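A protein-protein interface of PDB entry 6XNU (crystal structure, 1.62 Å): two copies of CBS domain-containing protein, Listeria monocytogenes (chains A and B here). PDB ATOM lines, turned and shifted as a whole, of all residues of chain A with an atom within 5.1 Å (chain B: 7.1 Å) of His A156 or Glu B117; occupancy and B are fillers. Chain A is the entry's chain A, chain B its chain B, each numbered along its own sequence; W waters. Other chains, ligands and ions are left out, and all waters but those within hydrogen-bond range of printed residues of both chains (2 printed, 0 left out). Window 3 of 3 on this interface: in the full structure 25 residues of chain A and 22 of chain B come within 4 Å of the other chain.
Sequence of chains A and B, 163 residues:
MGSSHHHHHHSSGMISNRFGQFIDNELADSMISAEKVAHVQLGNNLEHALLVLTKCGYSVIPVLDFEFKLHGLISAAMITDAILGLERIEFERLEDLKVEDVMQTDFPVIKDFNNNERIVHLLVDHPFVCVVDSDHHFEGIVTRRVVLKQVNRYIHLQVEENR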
ATOM      1  N   VAL A 151      -1.174  17.178   2.132  1.00  0.00           N
ATOM      2  CA  VAL A 151      -1.427  17.977   0.931  1.00  0.00           C
ATOM      3  C   VAL A 151      -0.112  18.353   0.257  1.00  0.00           C
ATOM      4  O   VAL A 151       0.030  18.266  -0.975  1.00  0.00           O
ATOM      5  CB  VAL A 151      -2.256  19.220   1.299  1.00  0.00           C
ATOM      6  CG1 VAL A 151      -2.311  20.191   0.128  1.00  0.00           C
ATOM      7  CG2 VAL A 151      -3.660  18.808   1.698  1.00  0.00           C
ATOM      8  N   ASN A 152       0.861  18.782   1.058  1.00  0.00           N
ATOM      9  CA  ASN A 152       2.218  19.061   0.592  1.00  0.00           C
ATOM     10  C   ASN A 152       2.797  17.863  -0.162  1.00  0.00           C
ATOM     11  O   ASN A 152       3.298  18.002  -1.283  1.00  0.00           O
ATOM     12  CB  ASN A 152       3.056  19.431   1.827  1.00  0.00           C
ATOM     13  CG  ASN A 152       4.421  19.964   1.505  1.00  0.00           C
ATOM     14  OD1 ASN A 152       4.574  21.034   0.898  1.00  0.00           O
ATOM     15  ND2 ASN A 152       5.445  19.230   1.945  1.00  0.00           N
ATOM     16  N   ARG A 153       2.693  16.666   0.423  1.00  0.00           N
ATOM     17  CA  ARG A 153       3.194  15.465  -0.245  1.00  0.00           C
ATOM     18  C   ARG A 153       2.469  15.231  -1.562  1.00  0.00           C
ATOM     19  O   ARG A 153       3.086  14.851  -2.570  1.00  0.00           O
ATOM     20  CB  ARG A 153       3.029  14.249   0.674  1.00  0.00           C
ATOM     21  CG  ARG A 153       3.577  12.961   0.097  1.00  0.00           C
ATOM     22  CD  ARG A 153       3.528  11.815   1.115  1.00  0.00           C
ATOM     23  NE  ARG A 153       2.162  11.437   1.475  1.00  0.00           N
ATOM     24  CZ  ARG A 153       1.621  11.607   2.685  1.00  0.00           C
ATOM     25  NH1 ARG A 153       2.322  12.159   3.672  1.00  0.00           N
ATOM     26  NH2 ARG A 153       0.368  11.225   2.909  1.00  0.00           N
ATOM     27  N   TYR A 154       1.157  15.447  -1.575  1.00  0.00           N
ATOM     28  CA  TYR A 154       0.392  15.202  -2.793  1.00  0.00           C
ATOM     29  C   TYR A 154       0.800  16.163  -3.906  1.00  0.00           C
ATOM     30  O   TYR A 154       0.955  15.748  -5.063  1.00  0.00           O
ATOM     31  CB  TYR A 154      -1.104  15.315  -2.506  1.00  0.00           C
ATOM     32  CG  TYR A 154      -1.971  15.039  -3.722  1.00  0.00           C
ATOM     33  CD1 TYR A 154      -2.146  13.744  -4.186  1.00  0.00           C
ATOM     34  CD2 TYR A 154      -2.632  16.069  -4.378  1.00  0.00           C
ATOM     35  CE1 TYR A 154      -2.934  13.481  -5.295  1.00  0.00           C
ATOM     36  CE2 TYR A 154      -3.427  15.815  -5.493  1.00  0.00           C
ATOM     37  CZ  TYR A 154      -3.577  14.521  -5.939  1.00  0.00           C
ATOM     38  OH  TYR A 154      -4.368  14.261  -7.044  1.00  0.00           O
ATOM     39  N   ILE A 155       0.975  17.444  -3.573  1.00  0.00           N
ATOM     40  CA  ILE A 155       1.413  18.432  -4.562  1.00  0.00           C
ATOM     41  C   ILE A 155       2.753  18.027  -5.158  1.00  0.00           C
ATOM     42  O   ILE A 155       2.980  18.170  -6.371  1.00  0.00           O
ATOM     43  CB  ILE A 155       1.468  19.829  -3.913  1.00  0.00           C
ATOM     44  CG1 ILE A 155       0.057  20.402  -3.790  1.00  0.00           C
ATOM     45  CG2 ILE A 155       2.390  20.775  -4.696  1.00  0.00           C
ATOM     46  CD1 ILE A 155      -0.032  21.586  -2.853  1.00  0.00           C
ATOM     47  N   HIS A 156       3.667  17.524  -4.327  1.00  0.00           N
ATOM     48  CA  HIS A 156       4.989  17.140  -4.816  1.00  0.00           C
ATOM     49  C   HIS A 156       4.923  15.875  -5.665  1.00  0.00           C
ATOM     50  O   HIS A 156       5.670  15.736  -6.642  1.00  0.00           O
ATOM     51  CB  HIS A 156       5.950  16.963  -3.642  1.00  0.00           C
ATOM     52  CG  HIS A 156       6.239  18.247  -2.918  1.00  0.00           C
ATOM     53  ND1 HIS A 156       6.549  18.303  -1.575  1.00  0.00           N
ATOM     54  CD2 HIS A 156       6.260  19.524  -3.366  1.00  0.00           C
ATOM     55  CE1 HIS A 156       6.744  19.566  -1.229  1.00  0.00           C
ATOM     56  NE2 HIS A 156       6.580  20.326  -2.298  1.00  0.00           N
ATOM     57  N   LEU A 157       4.036  14.949  -5.313  1.00  0.00           N
ATOM     58  CA  LEU A 157       3.849  13.768  -6.152  1.00  0.00           C
ATOM     59  C   LEU A 157       3.323  14.155  -7.526  1.00  0.00           C
ATOM     60  O   LEU A 157       3.706  13.549  -8.539  1.00  0.00           O
ATOM     61  CB  LEU A 157       2.902  12.792  -5.463  1.00  0.00           C
ATOM     62  CG  LEU A 157       3.489  12.144  -4.204  1.00  0.00           C
ATOM     63  CD1 LEU A 157       2.439  11.302  -3.504  1.00  0.00           C
ATOM     64  CD2 LEU A 157       4.728  11.314  -4.532  1.00  0.00           C
ATOM     65  N   GLN A 158       2.439  15.160  -7.583  1.00  0.00           N
ATOM     66  CA  GLN A 158       1.938  15.622  -8.879  1.00  0.00           C
ATOM     67  C   GLN A 158       3.062  16.203  -9.727  1.00  0.00           C
ATOM     68  O   GLN A 158       3.113  15.973 -10.943  1.00  0.00           O
ATOM     69  CB  GLN A 158       0.835  16.663  -8.695  1.00  0.00           C
ATOM     70  CG  GLN A 158      -0.425  16.120  -8.048  1.00  0.00           C
ATOM     71  CD  GLN A 158      -1.031  14.986  -8.843  1.00  0.00           C
ATOM     72  OE1 GLN A 158      -1.644  15.209  -9.878  1.00  0.00           O
ATOM     73  NE2 GLN A 158      -0.860  13.760  -8.361  1.00  0.00           N
ATOM     74  N   VAL A 159       3.962  16.965  -9.106  1.00  0.00           N
ATOM     75  CA  VAL A 159       5.143  17.446  -9.816  1.00  0.00           C
ATOM     76  C   VAL A 159       5.950  16.267 -10.348  1.00  0.00           C
ATOM     77  O   VAL A 159       6.353  16.253 -11.517  1.00  0.00           O
ATOM     78  CB  VAL A 159       5.977  18.355  -8.892  1.00  0.00           C
ATOM     79  CG1 VAL A 159       7.335  18.653  -9.496  1.00  0.00           C
ATOM     80  CG2 VAL A 159       5.206  19.643  -8.596  1.00  0.00           C
ATOM     81  N   GLU A 160       6.161  15.240  -9.513  1.00  0.00           N
ATOM     82  CA  GLU A 160       6.920  14.064  -9.950  1.00  0.00           C
ATOM     83  C   GLU A 160       6.243  13.359 -11.119  1.00  0.00           C
ATOM     84  O   GLU A 160       6.908  12.946 -12.080  1.00  0.00           O
ATOM     85  CB  GLU A 160       7.101  13.086  -8.783  1.00  0.00           C
ATOM     86  CG  GLU A 160       7.703  11.738  -9.178  1.00  0.00           C
ATOM     87  CD  GLU A 160       7.775  10.758  -8.014  1.00  0.00           C
ATOM     88  OE1 GLU A 160       7.211  11.056  -6.940  1.00  0.00           O
ATOM     89  OE2 GLU A 160       8.393   9.684  -8.175  1.00  0.00           O
ATOM     90  N   ASN B 114       2.156  33.868  -6.821  1.00  0.00           N
ATOM     91  CA  ASN B 114       2.950  33.378  -7.943  1.00  0.00           C
ATOM     92  C   ASN B 114       3.798  32.166  -7.588  1.00  0.00           C
ATOM     93  O   ASN B 114       4.436  31.585  -8.479  1.00  0.00           O
ATOM     94  CB  ASN B 114       3.839  34.504  -8.483  1.00  0.00           C
ATOM     95  CG  ASN B 114       3.034  35.615  -9.125  1.00  0.00           C
ATOM     96  OD1 ASN B 114       1.878  35.408  -9.515  1.00  0.00           O
ATOM     97  ND2 ASN B 114       3.637  36.792  -9.259  1.00  0.00           N
ATOM     98  N   ASN B 115       3.782  31.730  -6.317  1.00  0.00           N
ATOM     99  CA  ASN B 115       4.538  30.579  -5.868  1.00  0.00           C
ATOM    100  C   ASN B 115       3.629  29.761  -4.950  1.00  0.00           C
ATOM    101  O   ASN B 115       3.790  29.707  -3.727  1.00  0.00           O
ATOM    102  CB  ASN B 115       5.839  31.001  -5.183  1.00  0.00           C
ATOM    103  CG  ASN B 115       6.781  29.844  -4.966  1.00  0.00           C
ATOM    104  OD1 ASN B 115       6.394  28.683  -5.124  1.00  0.00           O
ATOM    105  ND2 ASN B 115       8.018  30.150  -4.565  1.00  0.00           N
ATOM    106  N   ASN B 116       2.641  29.104  -5.560  1.00  0.00           N
ATOM    107  CA  ASN B 116       1.645  28.383  -4.784  1.00  0.00           C
ATOM    108  C   ASN B 116       2.258  27.235  -3.991  1.00  0.00           C
ATOM    109  O   ASN B 116       1.801  26.946  -2.883  1.00  0.00           O
ATOM    110  CB  ASN B 116       0.531  27.868  -5.700  1.00  0.00           C
ATOM    111  CG  ASN B 116      -0.370  28.977  -6.205  1.00  0.00           C
ATOM    112  OD1 ASN B 116      -0.447  29.236  -7.411  1.00  0.00           O
ATOM    113  ND2 ASN B 116      -1.053  29.650  -5.281  1.00  0.00           N
ATOM    114  N   GLU B 117       3.294  26.577  -4.527  1.00  0.00           N
ATOM    115  CA  GLU B 117       3.924  25.488  -3.782  1.00  0.00           C
ATOM    116  C   GLU B 117       4.556  25.998  -2.494  1.00  0.00           C
ATOM    117  O   GLU B 117       4.511  25.318  -1.463  1.00  0.00           O
ATOM    118  CB  GLU B 117       4.977  24.786  -4.646  1.00  0.00           C
ATOM    119  CG  GLU B 117       5.584  23.534  -4.006  1.00  0.00           C
ATOM    120  CD  GLU B 117       6.735  23.824  -3.042  1.00  0.00           C
ATOM    121  OE1 GLU B 117       7.055  22.944  -2.222  1.00  0.00           O
ATOM    122  OE2 GLU B 117       7.326  24.931  -3.090  1.00  0.00           O
ATOM    123  N   ARG B 118       5.175  27.185  -2.541  1.00  0.00           N
ATOM    124  CA  ARG B 118       5.775  27.727  -1.321  1.00  0.00           C
ATOM    125  C   ARG B 118       4.715  28.043  -0.273  1.00  0.00           C
ATOM    126  O   ARG B 118       4.958  27.864   0.925  1.00  0.00           O
ATOM    127  CB  ARG B 118       6.605  28.982  -1.629  1.00  0.00           C
ATOM    128  CG  ARG B 118       7.300  29.562  -0.380  1.00  0.00           C
ATOM    129  CD  ARG B 118       8.019  30.875  -0.669  1.00  0.00           C
ATOM    130  NE  ARG B 118       8.574  31.446   0.561  1.00  0.00           N
ATOM    131  CZ  ARG B 118       8.083  32.510   1.184  1.00  0.00           C
ATOM    132  NH1 ARG B 118       7.021  33.142   0.701  1.00  0.00           N
ATOM    133  NH2 ARG B 118       8.658  32.940   2.300  1.00  0.00           N
ATOM    134  N   ILE B 119       3.542  28.526  -0.698  1.00  0.00           N
ATOM    135  CA  ILE B 119       2.489  28.869   0.262  1.00  0.00           C
ATOM    136  C   ILE B 119       2.031  27.627   1.025  1.00  0.00           C
ATOM    137  O   ILE B 119       1.920  27.644   2.253  1.00  0.00           O
ATOM    138  CB  ILE B 119       1.313  29.564  -0.448  1.00  0.00           C
ATOM    139  CG1 ILE B 119       1.779  30.866  -1.102  1.00  0.00           C
ATOM    140  CG2 ILE B 119       0.155  29.823   0.526  1.00  0.00           C
ATOM    141  CD1 ILE B 119       0.756  31.472  -2.034  1.00  0.00           C
ATOM    142  N   VAL B 120       1.768  26.524   0.309  1.00  0.00           N
ATOM    143  CA  VAL B 120       1.378  25.299   1.010  1.00  0.00           C
ATOM    144  C   VAL B 120       2.527  24.788   1.864  1.00  0.00           C
ATOM    145  O   VAL B 120       2.319  24.315   2.989  1.00  0.00           O
ATOM    146  CB  VAL B 120       0.904  24.233   0.009  1.00  0.00           C
ATOM    147  CG1 VAL B 120       0.608  22.930   0.742  1.00  0.00           C
ATOM    148  CG2 VAL B 120      -0.309  24.745  -0.754  1.00  0.00           C
ATOM    149  N   HIS B 121       3.766  24.908   1.367  1.00  0.00           N
ATOM    150  CA  HIS B 121       4.922  24.498   2.163  1.00  0.00           C
ATOM    151  C   HIS B 121       4.994  25.273   3.480  1.00  0.00           C
ATOM    152  O   HIS B 121       5.206  24.689   4.553  1.00  0.00           O
ATOM    153  CB  HIS B 121       6.204  24.677   1.341  1.00  0.00           C
ATOM    154  CG  HIS B 121       7.465  24.476   2.124  1.00  0.00           C
ATOM    155  ND1 HIS B 121       7.967  23.227   2.422  1.00  0.00           N
ATOM    156  CD2 HIS B 121       8.336  25.364   2.648  1.00  0.00           C
ATOM    157  CE1 HIS B 121       9.089  23.358   3.111  1.00  0.00           C
ATOM    158  NE2 HIS B 121       9.338  24.646   3.257  1.00  0.00           N
ATOM    159  N   LEU B 122       4.805  26.593   3.421  1.00  0.00           N
ATOM    160  CA  LEU B 122       4.825  27.399   4.639  1.00  0.00           C
ATOM    161  C   LEU B 122       3.724  26.982   5.604  1.00  0.00           C
ATOM    162  O   LEU B 122       3.908  27.032   6.828  1.00  0.00           O
ATOM    163  CB  LEU B 122       4.663  28.873   4.293  1.00  0.00           C
ATOM    164  CG  LEU B 122       5.853  29.531   3.636  1.00  0.00           C
ATOM    165  CD1 LEU B 122       5.420  30.896   3.183  1.00  0.00           C
ATOM    166  CD2 LEU B 122       6.971  29.629   4.663  1.00  0.00           C
ATOM    167  N   LEU B 123       2.556  26.623   5.079  1.00  0.00           N
ATOM    168  CA  LEU B 123       1.429  26.318   5.953  1.00  0.00           C
ATOM    169  C   LEU B 123       1.597  24.992   6.678  1.00  0.00           C
ATOM    170  O   LEU B 123       0.804  24.689   7.582  1.00  0.00           O
ATOM    171  CB  LEU B 123       0.133  26.321   5.147  1.00  0.00           C
ATOM    172  CG  LEU B 123      -0.352  27.698   4.696  1.00  0.00           C
ATOM    173  CD1 LEU B 123      -1.538  27.585   3.741  1.00  0.00           C
ATOM    174  CD2 LEU B 123      -0.714  28.536   5.940  1.00  0.00           C
HETATM  175  O   HOH W   1       3.657  22.480  -1.384  1.00  0.00           O
HETATM  176  O   HOH W   2       7.324  21.885   0.470  1.00  0.00           O
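No position is printed for both chains.
Of the 3 pairs that touch across the chains among the printed residues, none has its exchanged pair printed and touching as well.
Printed residues of chain B within 4 Å of Asn A152: His B121 (3.7 Å).
Printed residues of chain B within 4 Å of Ile A155: Val B120.
Of chain B, only Glu B117 (2.7 Å) comes within 4 Å of His A156.
Glu A160 touches none of the printed residues of chain B.
Of chain A, only His A156 comes within 4 Å of Glu B117.
Of the printed residues of chain A, Val B120 touches Ile A155.
Printed residues of chain A within 4 Å of His B121: Asn A152 (3.7 Å).
The nearest residue of chain B that does not touch His A156 is His B121 (5.3 Å).
The nearest residue of chain A that does not touch Glu B117 is Ile A155 (4.3 Å).
ND1 of His A156 is in hydrogen-bond range of O of Asn A152, at 3.3 Å.
Among the printed residues, pairs that only touch across the chains: Asn A152 with His B121 and Ile A155 with Val B120.
Water W2 lies within hydrogen-bond range of ND1 of His B121 (2.5 Å), OE1 of Glu B117 (2.9 Å), OD1 of Asn A152 (2.9 Å) and NE2 of His A156 (3.3 Å).
Water W1 lies within hydrogen-bond range of the side-chain amide oxygen of Asn A152 (2.9 Å) and the backbone carbonyl oxygen of Glu B117 (3.0 Å).
The side-chain carboxylate of Glu B117 sits at hydrogen-bond distance from a ring nitrogen (NE2) of His A156 (2.7 Å).
Of the 10 printed residues of chain A, 3 touch a printed residue of chain B.
Hydrophobic or aromatic side chains of chain A within 4 Å of the printed part of chain B: Ile A155 and His A156.
Printed residues of chain B that touch a printed residue of chain A: Glu B117, Val B120 and His B121.
Hydrophobic or aromatic side chains of chain B within 4 Å of the printed part of chain A: Val B120.
Along chain B the printed residues that touch a printed residue of chain A span positions 117 to 121.
Among the printed residues, no Asp or Glu carboxylate lies within 4 Å of a Lys or Arg side-chain nitrogen of the other chain.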
